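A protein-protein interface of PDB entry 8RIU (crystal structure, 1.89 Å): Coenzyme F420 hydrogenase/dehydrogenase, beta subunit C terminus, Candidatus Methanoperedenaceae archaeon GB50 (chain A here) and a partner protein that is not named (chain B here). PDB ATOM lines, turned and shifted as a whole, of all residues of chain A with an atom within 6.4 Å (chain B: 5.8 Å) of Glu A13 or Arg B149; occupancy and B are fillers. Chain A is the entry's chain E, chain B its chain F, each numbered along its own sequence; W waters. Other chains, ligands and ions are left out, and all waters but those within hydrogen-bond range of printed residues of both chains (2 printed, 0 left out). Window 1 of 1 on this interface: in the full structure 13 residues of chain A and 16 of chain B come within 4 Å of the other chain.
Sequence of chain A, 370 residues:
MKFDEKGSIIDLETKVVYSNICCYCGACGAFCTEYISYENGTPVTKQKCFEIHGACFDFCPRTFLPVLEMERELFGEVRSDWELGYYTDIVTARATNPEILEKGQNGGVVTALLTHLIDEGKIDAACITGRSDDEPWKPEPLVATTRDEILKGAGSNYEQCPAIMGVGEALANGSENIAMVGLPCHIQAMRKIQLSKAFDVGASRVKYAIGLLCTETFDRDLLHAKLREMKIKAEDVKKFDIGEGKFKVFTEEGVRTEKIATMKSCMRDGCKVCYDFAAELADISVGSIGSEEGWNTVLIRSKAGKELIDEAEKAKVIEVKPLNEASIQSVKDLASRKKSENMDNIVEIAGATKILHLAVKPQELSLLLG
The side-chain hydroxyl (OG) of Ser A8 is in hydrogen-bond range of the guanidinium group (NH2) of Arg B17, 3.5 Å away. The side-chain carboxylate (OD1) of Asp A11 is in salt-bridge range of the guanidinium group (NE) of Arg B17 (3.0 Å). The guanidinium group (NH2) of Arg B136 is in salt-bridge range of the side-chain carboxylate (OE2) of Glu A13, at 2.8 Å. The guanidinium group (NE) of Arg B149 is in salt-bridge range of the side-chain carboxylate (OE1) of Glu A13, 3.1 Å away. The side-chain sulfur (SD) of Met B150 lies close to the side-chain hydroxyl (OG1) of Thr A14, 3.4 Å away. The guanidinium group (NH2) of Arg B136 lies within hydrogen-bond range of the side-chain hydroxyl (OG1) of Thr A45, 3.0 Å away. The side-chain carboxylate (OE1) of Glu B14 is in salt-bridge range of the side-chain amino group (NZ) of Lys A48.
The backbone NH (N) of Ser A8 sits at hydrogen-bond distance from the side-chain carboxylate (OD2) of Asp A11, 2.8 Å away. The backbone carbonyl oxygen (O) of Ile A10 sits at hydrogen-bond distance from the side-chain hydroxyl (OG1) of Thr A14, 2.8 Å away. The backbone carbonyl oxygen (O) of Thr A14 sits at hydrogen-bond distance from the side-chain hydroxyl (OG) of Ser A19. NH1 of Arg B17 lies within hydrogen-bond range of O of Met B15. The backbone NH (N) of Arg B17 lies within hydrogen-bond range of the backbone carbonyl oxygen (O) of Arg B149, 3.1 Å away. The backbone carbonyl oxygen (O) of Arg B17 lies within hydrogen-bond range of the backbone NH (N) of Thr B151 (2.9 Å).
Among the printed residues, merely in contact across the chains: Tyr A18 with Ala B23, Tyr A18 with Met B150, Ile A10 with Arg B149, Ile A10 with Arg B17, Tyr A18 with Arg B136, Thr A14 with Arg B17, Thr A45 with Leu B134, Ile A10 with Glu B14 and Ile A9 with Arg B149.
Printed residues of chain A within 4 Å of Arg B149: Ile A9 (3.99 Å), Ile A10 (3.5 Å) and Glu A13 (3.1 Å). Printed residues of chain A within 4 Å of Arg B136: Glu A13 (2.8 Å), Tyr A18 (3.6 Å) and Thr A45 (3.0 Å). Printed residues of chain B within 4 Å of Ser A8: Arg B17 (3.5 Å). The nearest residue of chain B that does not touch Glu A13 is Met B150 (4.7 Å). The nearest printed residue of chain A that does not touch Arg B149 is Thr A45 (4.7 Å).
Printed residues of chain A that touch a printed residue of chain B: Ser A8, Ile A9, Ile A10, Asp A11, Glu A13, Thr A14, Tyr A18, Thr A45 and Lys A48. Hydrophobic or aromatic side chains of chain A that line the printed part of chain B: Ile A9, Ile A10 and Tyr A18. Of the 16 printed residues of chain B, 7 touch a printed residue of chain A. Printed residues of chain B that touch a printed residue of chain A: Glu B14, Arg B17, Ala B23, Leu B134, Arg B136, Arg B149 and Met B150. Hydrophobic or aromatic side chains of chain B that line the printed part of chain A: Ala B23, Leu B134 and Met B150. Among the printed residues, Asp or Glu carboxylates within 4 Å of a Lys or Arg side-chain nitrogen of the other chain: Asp A11 with Arg B17 (3.0 Å), Glu A13 with Arg B136 (2.8 Å), Glu A13 with Arg B149 (3.1 Å) and Lys A48 with Glu B14 (2.7 Å).
Water W1 lies within hydrogen-bond range of OE1 of Glu A13 (2.5 Å), NE of Arg B149 (3.2 Å) and SD of Met B150 (3.5 Å). Water W2 lies within hydrogen-bond range of the side-chain carboxylate (OE2) of Glu B14 and the side-chain hydroxyl (OG) of Ser A8.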
ATOM      1  N   SER A   8     -26.042   0.307  20.962  1.00  0.00           N
ATOM      2  CA  SER A   8     -24.894   0.438  20.080  1.00  0.00           C
ATOM      3  C   SER A   8     -24.972   1.785  19.362  1.00  0.00           C
ATOM      4  O   SER A   8     -25.815   2.634  19.676  1.00  0.00           O
ATOM      5  CB  SER A   8     -24.842  -0.736  19.094  1.00  0.00           C
ATOM      6  OG  SER A   8     -25.771  -0.544  18.033  1.00  0.00           O
ATOM      7  N   ILE A   9     -24.081   1.973  18.384  1.00  0.00           N
ATOM      8  CA  ILE A   9     -23.979   3.261  17.701  1.00  0.00           C
ATOM      9  C   ILE A   9     -25.300   3.626  17.039  1.00  0.00           C
ATOM     10  O   ILE A   9     -25.677   4.803  16.987  1.00  0.00           O
ATOM     11  CB  ILE A   9     -22.821   3.235  16.681  1.00  0.00           C
ATOM     12  CG1 ILE A   9     -22.735   4.564  15.918  1.00  0.00           C
ATOM     13  CG2 ILE A   9     -22.982   2.076  15.692  1.00  0.00           C
ATOM     14  CD1 ILE A   9     -22.473   5.769  16.798  1.00  0.00           C
ATOM     15  N   ILE A  10     -26.017   2.636  16.509  1.00  0.00           N
ATOM     16  CA  ILE A  10     -27.277   2.934  15.832  1.00  0.00           C
ATOM     17  C   ILE A  10     -28.281   3.497  16.826  1.00  0.00           C
ATOM     18  O   ILE A  10     -29.031   4.429  16.515  1.00  0.00           O
ATOM     19  CB  ILE A  10     -27.822   1.680  15.125  1.00  0.00           C
ATOM     20  CG1 ILE A  10     -26.840   1.199  14.052  1.00  0.00           C
ATOM     21  CG2 ILE A  10     -29.187   1.970  14.495  1.00  0.00           C
ATOM     22  CD1 ILE A  10     -27.134  -0.227  13.519  1.00  0.00           C
ATOM     23  N   ASP A  11     -28.321   2.934  18.033  1.00  0.00           N
ATOM     24  CA  ASP A  11     -29.201   3.483  19.055  1.00  0.00           C
ATOM     25  C   ASP A  11     -28.775   4.890  19.439  1.00  0.00           C
ATOM     26  O   ASP A  11     -29.623   5.765  19.644  1.00  0.00           O
ATOM     27  CB  ASP A  11     -29.216   2.570  20.274  1.00  0.00           C
ATOM     28  CG  ASP A  11     -29.584   1.154  19.922  1.00  0.00           C
ATOM     29  OD1 ASP A  11     -30.777   0.910  19.625  1.00  0.00           O
ATOM     30  OD2 ASP A  11     -28.679   0.285  19.943  1.00  0.00           O
ATOM     31  N   LEU A  12     -27.464   5.126  19.543  1.00  0.00           N
ATOM     32  CA  LEU A  12     -26.981   6.466  19.860  1.00  0.00           C
ATOM     33  C   LEU A  12     -27.404   7.461  18.792  1.00  0.00           C
ATOM     34  O   LEU A  12     -27.834   8.577  19.108  1.00  0.00           O
ATOM     35  CB  LEU A  12     -25.457   6.464  20.001  1.00  0.00           C
ATOM     36  CG  LEU A  12     -24.839   7.822  20.348  1.00  0.00           C
ATOM     37  CD1 LEU A  12     -25.206   8.228  21.767  1.00  0.00           C
ATOM     38  CD2 LEU A  12     -23.335   7.817  20.152  1.00  0.00           C
ATOM     39  N   GLU A  13     -27.281   7.082  17.519  1.00  0.00           N
ATOM     40  CA  GLU A  13     -27.710   7.971  16.445  1.00  0.00           C
ATOM     41  C   GLU A  13     -29.217   8.179  16.477  1.00  0.00           C
ATOM     42  O   GLU A  13     -29.701   9.297  16.262  1.00  0.00           O
ATOM     43  CB  GLU A  13     -27.267   7.405  15.097  1.00  0.00           C
ATOM     44  CG  GLU A  13     -25.752   7.419  14.935  1.00  0.00           C
ATOM     45  CD  GLU A  13     -25.275   6.745  13.674  1.00  0.00           C
ATOM     46  OE1 GLU A  13     -26.115   6.263  12.878  1.00  0.00           O
ATOM     47  OE2 GLU A  13     -24.040   6.684  13.486  1.00  0.00           O
ATOM     48  N   THR A  14     -29.975   7.119  16.767  1.00  0.00           N
ATOM     49  CA  THR A  14     -31.431   7.220  16.739  1.00  0.00           C
ATOM     50  C   THR A  14     -31.956   8.094  17.874  1.00  0.00           C
ATOM     51  O   THR A  14     -32.840   8.932  17.663  1.00  0.00           O
ATOM     52  CB  THR A  14     -32.044   5.819  16.807  1.00  0.00           C
ATOM     53  OG1 THR A  14     -31.633   5.058  15.662  1.00  0.00           O
ATOM     54  CG2 THR A  14     -33.564   5.883  16.839  1.00  0.00           C
ATOM     55  N   LYS A  15     -31.419   7.924  19.081  1.00  0.00           N
ATOM     56  CA  LYS A  15     -31.983   8.573  20.255  1.00  0.00           C
ATOM     57  C   LYS A  15     -31.320   9.896  20.603  1.00  0.00           C
ATOM     58  O   LYS A  15     -31.931  10.701  21.313  1.00  0.00           O
ATOM     59  CB  LYS A  15     -31.882   7.644  21.469  1.00  0.00           C
ATOM     60  CG  LYS A  15     -32.669   6.351  21.331  1.00  0.00           C
ATOM     61  CD  LYS A  15     -34.176   6.598  21.406  1.00  0.00           C
ATOM     62  CE  LYS A  15     -34.947   5.307  21.171  1.00  0.00           C
ATOM     63  NZ  LYS A  15     -36.416   5.540  21.073  1.00  0.00           N
ATOM     64  N   VAL A  16     -30.105  10.147  20.119  1.00  0.00           N
ATOM     65  CA  VAL A  16     -29.331  11.298  20.572  1.00  0.00           C
ATOM     66  C   VAL A  16     -28.936  12.153  19.373  1.00  0.00           C
ATOM     67  O   VAL A  16     -29.418  13.280  19.224  1.00  0.00           O
ATOM     68  CB  VAL A  16     -28.107  10.830  21.384  1.00  0.00           C
ATOM     69  CG1 VAL A  16     -27.210  12.000  21.763  1.00  0.00           C
ATOM     70  CG2 VAL A  16     -28.571  10.080  22.625  1.00  0.00           C
ATOM     71  N   VAL A  17     -28.067  11.626  18.507  1.00  0.00           N
ATOM     72  CA  VAL A  17     -27.502  12.442  17.431  1.00  0.00           C
ATOM     73  C   VAL A  17     -28.595  13.018  16.540  1.00  0.00           C
ATOM     74  O   VAL A  17     -28.701  14.237  16.359  1.00  0.00           O
ATOM     75  CB  VAL A  17     -26.493  11.623  16.606  1.00  0.00           C
ATOM     76  CG1 VAL A  17     -25.857  12.497  15.516  1.00  0.00           C
ATOM     77  CG2 VAL A  17     -25.417  11.034  17.507  1.00  0.00           C
ATOM     78  N   TYR A  18     -29.401  12.146  15.943  1.00  0.00           N
ATOM     79  CA  TYR A  18     -30.445  12.589  15.037  1.00  0.00           C
ATOM     80  C   TYR A  18     -31.656  13.142  15.770  1.00  0.00           C
ATOM     81  O   TYR A  18     -32.522  13.741  15.125  1.00  0.00           O
ATOM     82  CB  TYR A  18     -30.846  11.433  14.122  1.00  0.00           C
ATOM     83  CG  TYR A  18     -29.749  11.035  13.155  1.00  0.00           C
ATOM     84  CD1 TYR A  18     -28.984  11.999  12.510  1.00  0.00           C
ATOM     85  CD2 TYR A  18     -29.470   9.698  12.896  1.00  0.00           C
ATOM     86  CE1 TYR A  18     -27.981  11.649  11.626  1.00  0.00           C
ATOM     87  CE2 TYR A  18     -28.469   9.335  12.008  1.00  0.00           C
ATOM     88  CZ  TYR A  18     -27.726  10.320  11.377  1.00  0.00           C
ATOM     89  OH  TYR A  18     -26.731   9.989  10.484  1.00  0.00           O
ATOM     90  N   SER A  19     -31.731  12.970  17.092  1.00  0.00           N
ATOM     91  CA  SER A  19     -32.745  13.629  17.906  1.00  0.00           C
ATOM     92  C   SER A  19     -32.357  15.053  18.272  1.00  0.00           C
ATOM     93  O   SER A  19     -33.184  15.774  18.837  1.00  0.00           O
ATOM     94  CB  SER A  19     -32.995  12.839  19.192  1.00  0.00           C
ATOM     95  OG  SER A  19     -33.769  11.684  18.933  1.00  0.00           O
ATOM     96  N   PRO A  43     -20.964  13.231  17.155  1.00  0.00           N
ATOM     97  CA  PRO A  43     -20.151  12.079  16.758  1.00  0.00           C
ATOM     98  C   PRO A  43     -20.590  11.495  15.427  1.00  0.00           C
ATOM     99  O   PRO A  43     -21.767  11.518  15.054  1.00  0.00           O
ATOM    100  CB  PRO A  43     -20.367  11.080  17.900  1.00  0.00           C
ATOM    101  CG  PRO A  43     -21.716  11.430  18.439  1.00  0.00           C
ATOM    102  CD  PRO A  43     -21.869  12.911  18.275  1.00  0.00           C
ATOM    103  N   VAL A  44     -19.604  10.989  14.692  1.00  0.00           N
ATOM    104  CA  VAL A  44     -19.833  10.258  13.457  1.00  0.00           C
ATOM    105  C   VAL A  44     -18.904   9.055  13.454  1.00  0.00           C
ATOM    106  O   VAL A  44     -17.876   9.032  14.136  1.00  0.00           O
ATOM    107  CB  VAL A  44     -19.593  11.128  12.206  1.00  0.00           C
ATOM    108  CG1 VAL A  44     -20.507  12.339  12.227  1.00  0.00           C
ATOM    109  CG2 VAL A  44     -18.143  11.574  12.134  1.00  0.00           C
ATOM    110  N   THR A  45     -19.294   8.039  12.691  1.00  0.00           N
ATOM    111  CA  THR A  45     -18.412   6.939  12.335  1.00  0.00           C
ATOM    112  C   THR A  45     -18.371   6.834  10.817  1.00  0.00           C
ATOM    113  O   THR A  45     -19.337   7.190  10.131  1.00  0.00           O
ATOM    114  CB  THR A  45     -18.864   5.607  12.946  1.00  0.00           C
ATOM    115  OG1 THR A  45     -20.054   5.143  12.294  1.00  0.00           O
ATOM    116  CG2 THR A  45     -19.122   5.755  14.433  1.00  0.00           C
ATOM    117  N   LYS A  48     -18.261   0.664   9.375  1.00  0.00           N
ATOM    118  CA  LYS A  48     -19.165  -0.139  10.219  1.00  0.00           C
ATOM    119  C   LYS A  48     -18.401  -0.776  11.375  1.00  0.00           C
ATOM    120  O   LYS A  48     -17.292  -1.247  11.152  1.00  0.00           O
ATOM    121  CB  LYS A  48     -19.876  -1.235   9.422  1.00  0.00           C
ATOM    122  CG  LYS A  48     -20.869  -2.074  10.211  1.00  0.00           C
ATOM    123  CD  LYS A  48     -21.747  -2.941   9.343  1.00  0.00           C
ATOM    124  CE  LYS A  48     -22.860  -3.612  10.115  1.00  0.00           C
ATOM    125  NZ  LYS A  48     -23.679  -2.629  10.859  1.00  0.00           N
ATOM    126  N   CYS A  49     -18.969  -0.701  12.565  1.00  0.00           N
ATOM    127  CA  CYS A  49     -18.438  -1.390  13.731  1.00  0.00           C
ATOM    128  C   CYS A  49     -19.307  -2.610  14.033  1.00  0.00           C
ATOM    129  O   CYS A  49     -20.405  -2.777  13.495  1.00  0.00           O
ATOM    130  CB  CYS A  49     -18.365  -0.448  14.939  1.00  0.00           C
ATOM    131  SG  CYS A  49     -19.904   0.381  15.404  1.00  0.00           S
ATOM    132  N   GLU B  14     -29.118  -7.748  14.012  1.00  0.00           N
ATOM    133  CA  GLU B  14     -29.021  -6.287  13.954  1.00  0.00           C
ATOM    134  C   GLU B  14     -30.264  -5.777  13.240  1.00  0.00           C
ATOM    135  O   GLU B  14     -30.336  -5.780  12.009  1.00  0.00           O
ATOM    136  CB  GLU B  14     -27.754  -5.838  13.240  1.00  0.00           C
ATOM    137  CG  GLU B  14     -27.514  -4.333  13.307  1.00  0.00           C
ATOM    138  CD  GLU B  14     -26.152  -3.948  12.754  1.00  0.00           C
ATOM    139  OE1 GLU B  14     -26.051  -3.720  11.528  1.00  0.00           O
ATOM    140  OE2 GLU B  14     -25.182  -3.876  13.542  1.00  0.00           O
ATOM    141  N   MET B  15     -31.222  -5.305  14.017  1.00  0.00           N
ATOM    142  CA  MET B  15     -32.579  -5.072  13.562  1.00  0.00           C
ATOM    143  C   MET B  15     -32.815  -3.571  13.524  1.00  0.00           C
ATOM    144  O   MET B  15     -32.339  -2.846  14.404  1.00  0.00           O
ATOM    145  CB  MET B  15     -33.549  -5.766  14.513  1.00  0.00           C
ATOM    146  CG  MET B  15     -33.460  -7.278  14.410  1.00  0.00           C
ATOM    147  SD  MET B  15     -34.819  -8.208  15.152  1.00  0.00           S
ATOM    148  CE  MET B  15     -35.099  -7.353  16.686  1.00  0.00           C
ATOM    149  N   GLY B  16     -33.531  -3.106  12.504  1.00  0.00           N
ATOM    150  CA  GLY B  16     -33.668  -1.671  12.306  1.00  0.00           C
ATOM    151  C   GLY B  16     -34.362  -1.000  13.479  1.00  0.00           C
ATOM    152  O   GLY B  16     -35.296  -1.544  14.071  1.00  0.00           O
ATOM    153  N   ARG B  17     -33.903   0.212  13.803  1.00  0.00           N
ATOM    154  CA  ARG B  17     -34.376   0.944  14.972  1.00  0.00           C
ATOM    155  C   ARG B  17     -35.553   1.839  14.606  1.00  0.00           C
ATOM    156  O   ARG B  17     -35.504   2.556  13.603  1.00  0.00           O
ATOM    157  CB  ARG B  17     -33.248   1.800  15.555  1.00  0.00           C
ATOM    158  CG  ARG B  17     -32.422   1.112  16.616  1.00  0.00           C
ATOM    159  CD  ARG B  17     -31.665  -0.094  16.073  1.00  0.00           C
ATOM    160  NE  ARG B  17     -30.614  -0.500  16.999  1.00  0.00           N
ATOM    161  CZ  ARG B  17     -29.901  -1.613  16.893  1.00  0.00           C
ATOM    162  NH1 ARG B  17     -30.106  -2.473  15.910  1.00  0.00           N
ATOM    163  NH2 ARG B  17     -28.961  -1.867  17.798  1.00  0.00           N
ATOM    164  N   ALA B  23     -36.183  12.567  13.540  1.00  0.00           N
ATOM    165  CA  ALA B  23     -34.843  11.994  13.532  1.00  0.00           C
ATOM    166  C   ALA B  23     -34.468  11.526  12.135  1.00  0.00           C
ATOM    167  O   ALA B  23     -33.323  11.698  11.701  1.00  0.00           O
ATOM    168  CB  ALA B  23     -34.760  10.841  14.530  1.00  0.00           C
ATOM    169  N   LEU B 134     -18.786   3.687   5.240  1.00  0.00           N
ATOM    170  CA  LEU B 134     -20.117   3.312   5.692  1.00  0.00           C
ATOM    171  C   LEU B 134     -21.169   4.173   5.005  1.00  0.00           C
ATOM    172  O   LEU B 134     -21.068   5.404   4.976  1.00  0.00           O
ATOM    173  CB  LEU B 134     -20.217   3.458   7.211  1.00  0.00           C
ATOM    174  CG  LEU B 134     -21.616   3.358   7.824  1.00  0.00           C
ATOM    175  CD1 LEU B 134     -22.133   1.937   7.704  1.00  0.00           C
ATOM    176  CD2 LEU B 134     -21.605   3.794   9.281  1.00  0.00           C
ATOM    177  N   VAL B 135     -22.174   3.514   4.442  1.00  0.00           N
ATOM    178  CA  VAL B 135     -23.362   4.161   3.908  1.00  0.00           C
ATOM    179  C   VAL B 135     -24.513   3.830   4.846  1.00  0.00           C
ATOM    180  O   VAL B 135     -24.777   2.653   5.116  1.00  0.00           O
ATOM    181  CB  VAL B 135     -23.674   3.691   2.476  1.00  0.00           C
ATOM    182  CG1 VAL B 135     -24.939   4.360   1.959  1.00  0.00           C
ATOM    183  CG2 VAL B 135     -22.508   3.970   1.546  1.00  0.00           C
ATOM    184  N   ARG B 136     -25.189   4.858   5.341  1.00  0.00           N
ATOM    185  CA  ARG B 136     -26.336   4.680   6.223  1.00  0.00           C
ATOM    186  C   ARG B 136     -27.603   4.650   5.381  1.00  0.00           C
ATOM    187  O   ARG B 136     -27.862   5.584   4.620  1.00  0.00           O
ATOM    188  CB  ARG B 136     -26.399   5.808   7.248  1.00  0.00           C
ATOM    189  CG  ARG B 136     -25.332   5.727   8.326  1.00  0.00           C
ATOM    190  CD  ARG B 136     -25.203   7.043   9.065  1.00  0.00           C
ATOM    191  NE  ARG B 136     -24.323   6.927  10.220  1.00  0.00           N
ATOM    192  CZ  ARG B 136     -23.000   6.944  10.159  1.00  0.00           C
ATOM    193  NH1 ARG B 136     -22.361   7.089   9.008  1.00  0.00           N
ATOM    194  NH2 ARG B 136     -22.300   6.807  11.279  1.00  0.00           N
ATOM    195  N   ALA B 137     -28.388   3.587   5.509  1.00  0.00           N
ATOM    196  CA  ALA B 137     -29.647   3.468   4.785  1.00  0.00           C
ATOM    197  C   ALA B 137     -30.799   3.481   5.775  1.00  0.00           C
ATOM    198  O   ALA B 137     -30.769   2.760   6.779  1.00  0.00           O
ATOM    199  CB  ALA B 137     -29.687   2.198   3.934  1.00  0.00           C
ATOM    200  N   ILE B 138     -31.809   4.305   5.487  1.00  0.00           N
ATOM    201  CA  ILE B 138     -32.966   4.489   6.347  1.00  0.00           C
ATOM    202  C   ILE B 138     -34.230   4.321   5.513  1.00  0.00           C
ATOM    203  O   ILE B 138     -34.209   4.372   4.282  1.00  0.00           O
ATOM    204  CB  ILE B 138     -32.966   5.872   7.050  1.00  0.00           C
ATOM    205  CG1 ILE B 138     -33.146   7.002   6.035  1.00  0.00           C
ATOM    206  CG2 ILE B 138     -31.679   6.069   7.830  1.00  0.00           C
ATOM    207  CD1 ILE B 138     -33.309   8.382   6.662  1.00  0.00           C
ATOM    208  N   HIS B 145     -38.857  -1.558   8.221  1.00  0.00           N
ATOM    209  CA  HIS B 145     -37.778  -2.093   7.396  1.00  0.00           C
ATOM    210  C   HIS B 145     -36.692  -2.570   8.348  1.00  0.00           C
ATOM    211  O   HIS B 145     -35.794  -1.819   8.735  1.00  0.00           O
ATOM    212  CB  HIS B 145     -37.292  -1.059   6.386  1.00  0.00           C
ATOM    213  CG  HIS B 145     -37.975  -1.177   5.062  1.00  0.00           C
ATOM    214  ND1 HIS B 145     -37.936  -2.334   4.314  1.00  0.00           N
ATOM    215  CD2 HIS B 145     -38.728  -0.299   4.358  1.00  0.00           C
ATOM    216  CE1 HIS B 145     -38.638  -2.166   3.207  1.00  0.00           C
ATOM    217  NE2 HIS B 145     -39.128  -0.938   3.209  1.00  0.00           N
ATOM    218  N   ALA B 147     -34.298  -4.293   7.789  1.00  0.00           N
ATOM    219  CA  ALA B 147     -32.985  -4.219   7.168  1.00  0.00           C
ATOM    220  C   ALA B 147     -32.468  -2.794   7.070  1.00  0.00           C
ATOM    221  O   ALA B 147     -31.314  -2.593   6.681  1.00  0.00           O
ATOM    222  CB  ALA B 147     -33.027  -4.838   5.766  1.00  0.00           C
ATOM    223  N   ALA B 148     -33.296  -1.808   7.391  1.00  0.00           N
ATOM    224  CA  ALA B 148     -32.817  -0.442   7.453  1.00  0.00           C
ATOM    225  C   ALA B 148     -32.090  -0.203   8.768  1.00  0.00           C
ATOM    226  O   ALA B 148     -32.250  -0.943   9.748  1.00  0.00           O
ATOM    227  CB  ALA B 148     -33.966   0.555   7.318  1.00  0.00           C
ATOM    228  N   ARG B 149     -31.274   0.850   8.769  1.00  0.00           N
ATOM    229  CA  ARG B 149     -30.662   1.329  10.001  1.00  0.00           C
ATOM    230  C   ARG B 149     -31.709   1.939  10.917  1.00  0.00           C
ATOM    231  O   ARG B 149     -31.770   1.627  12.113  1.00  0.00           O
ATOM    232  CB  ARG B 149     -29.595   2.364   9.656  1.00  0.00           C
ATOM    233  CG  ARG B 149     -28.446   2.426  10.604  1.00  0.00           C
ATOM    234  CD  ARG B 149     -27.391   3.375  10.070  1.00  0.00           C
ATOM    235  NE  ARG B 149     -26.431   3.754  11.100  1.00  0.00           N
ATOM    236  CZ  ARG B 149     -25.337   3.066  11.393  1.00  0.00           C
ATOM    237  NH1 ARG B 149     -25.066   1.916  10.794  1.00  0.00           N
ATOM    238  NH2 ARG B 149     -24.491   3.546  12.302  1.00  0.00           N
ATOM    239  N   MET B 150     -32.481   2.859  10.357  1.00  0.00           N
ATOM    240  CA  MET B 150     -33.566   3.518  11.114  1.00  0.00           C
ATOM    241  C   MET B 150     -34.817   3.441  10.244  1.00  0.00           C
ATOM    242  O   MET B 150     -34.679   3.483   9.017  1.00  0.00           O
ATOM    243  CB  MET B 150     -33.207   4.971  11.416  1.00  0.00           C
ATOM    244  CG  MET B 150     -32.117   5.132  12.447  1.00  0.00           C
ATOM    245  SD  MET B 150     -31.790   6.876  12.761  1.00  0.00           S
ATOM    246  CE  MET B 150     -31.420   7.432  11.101  1.00  0.00           C
ATOM    247  N   THR B 151     -35.980   3.311  10.863  1.00  0.00           N
ATOM    248  CA  THR B 151     -37.221   3.119  10.085  1.00  0.00           C
ATOM    249  C   THR B 151     -38.439   3.473  10.921  1.00  0.00           C
ATOM    250  O   THR B 151     -38.301   3.644  12.126  1.00  0.00           O
ATOM    251  CB  THR B 151     -37.385   1.652   9.676  1.00  0.00           C
ATOM    252  OG1 THR B 151     -38.656   1.450   9.058  1.00  0.00           O
ATOM    253  CG2 THR B 151     -37.237   0.711  10.850  1.00  0.00           C
HETATM  254  O   HOH W   1     -28.501   5.697  12.505  1.00  0.00           O
HETATM  255  O   HOH W   2     -24.306  -1.422  15.188  1.00  0.00           O
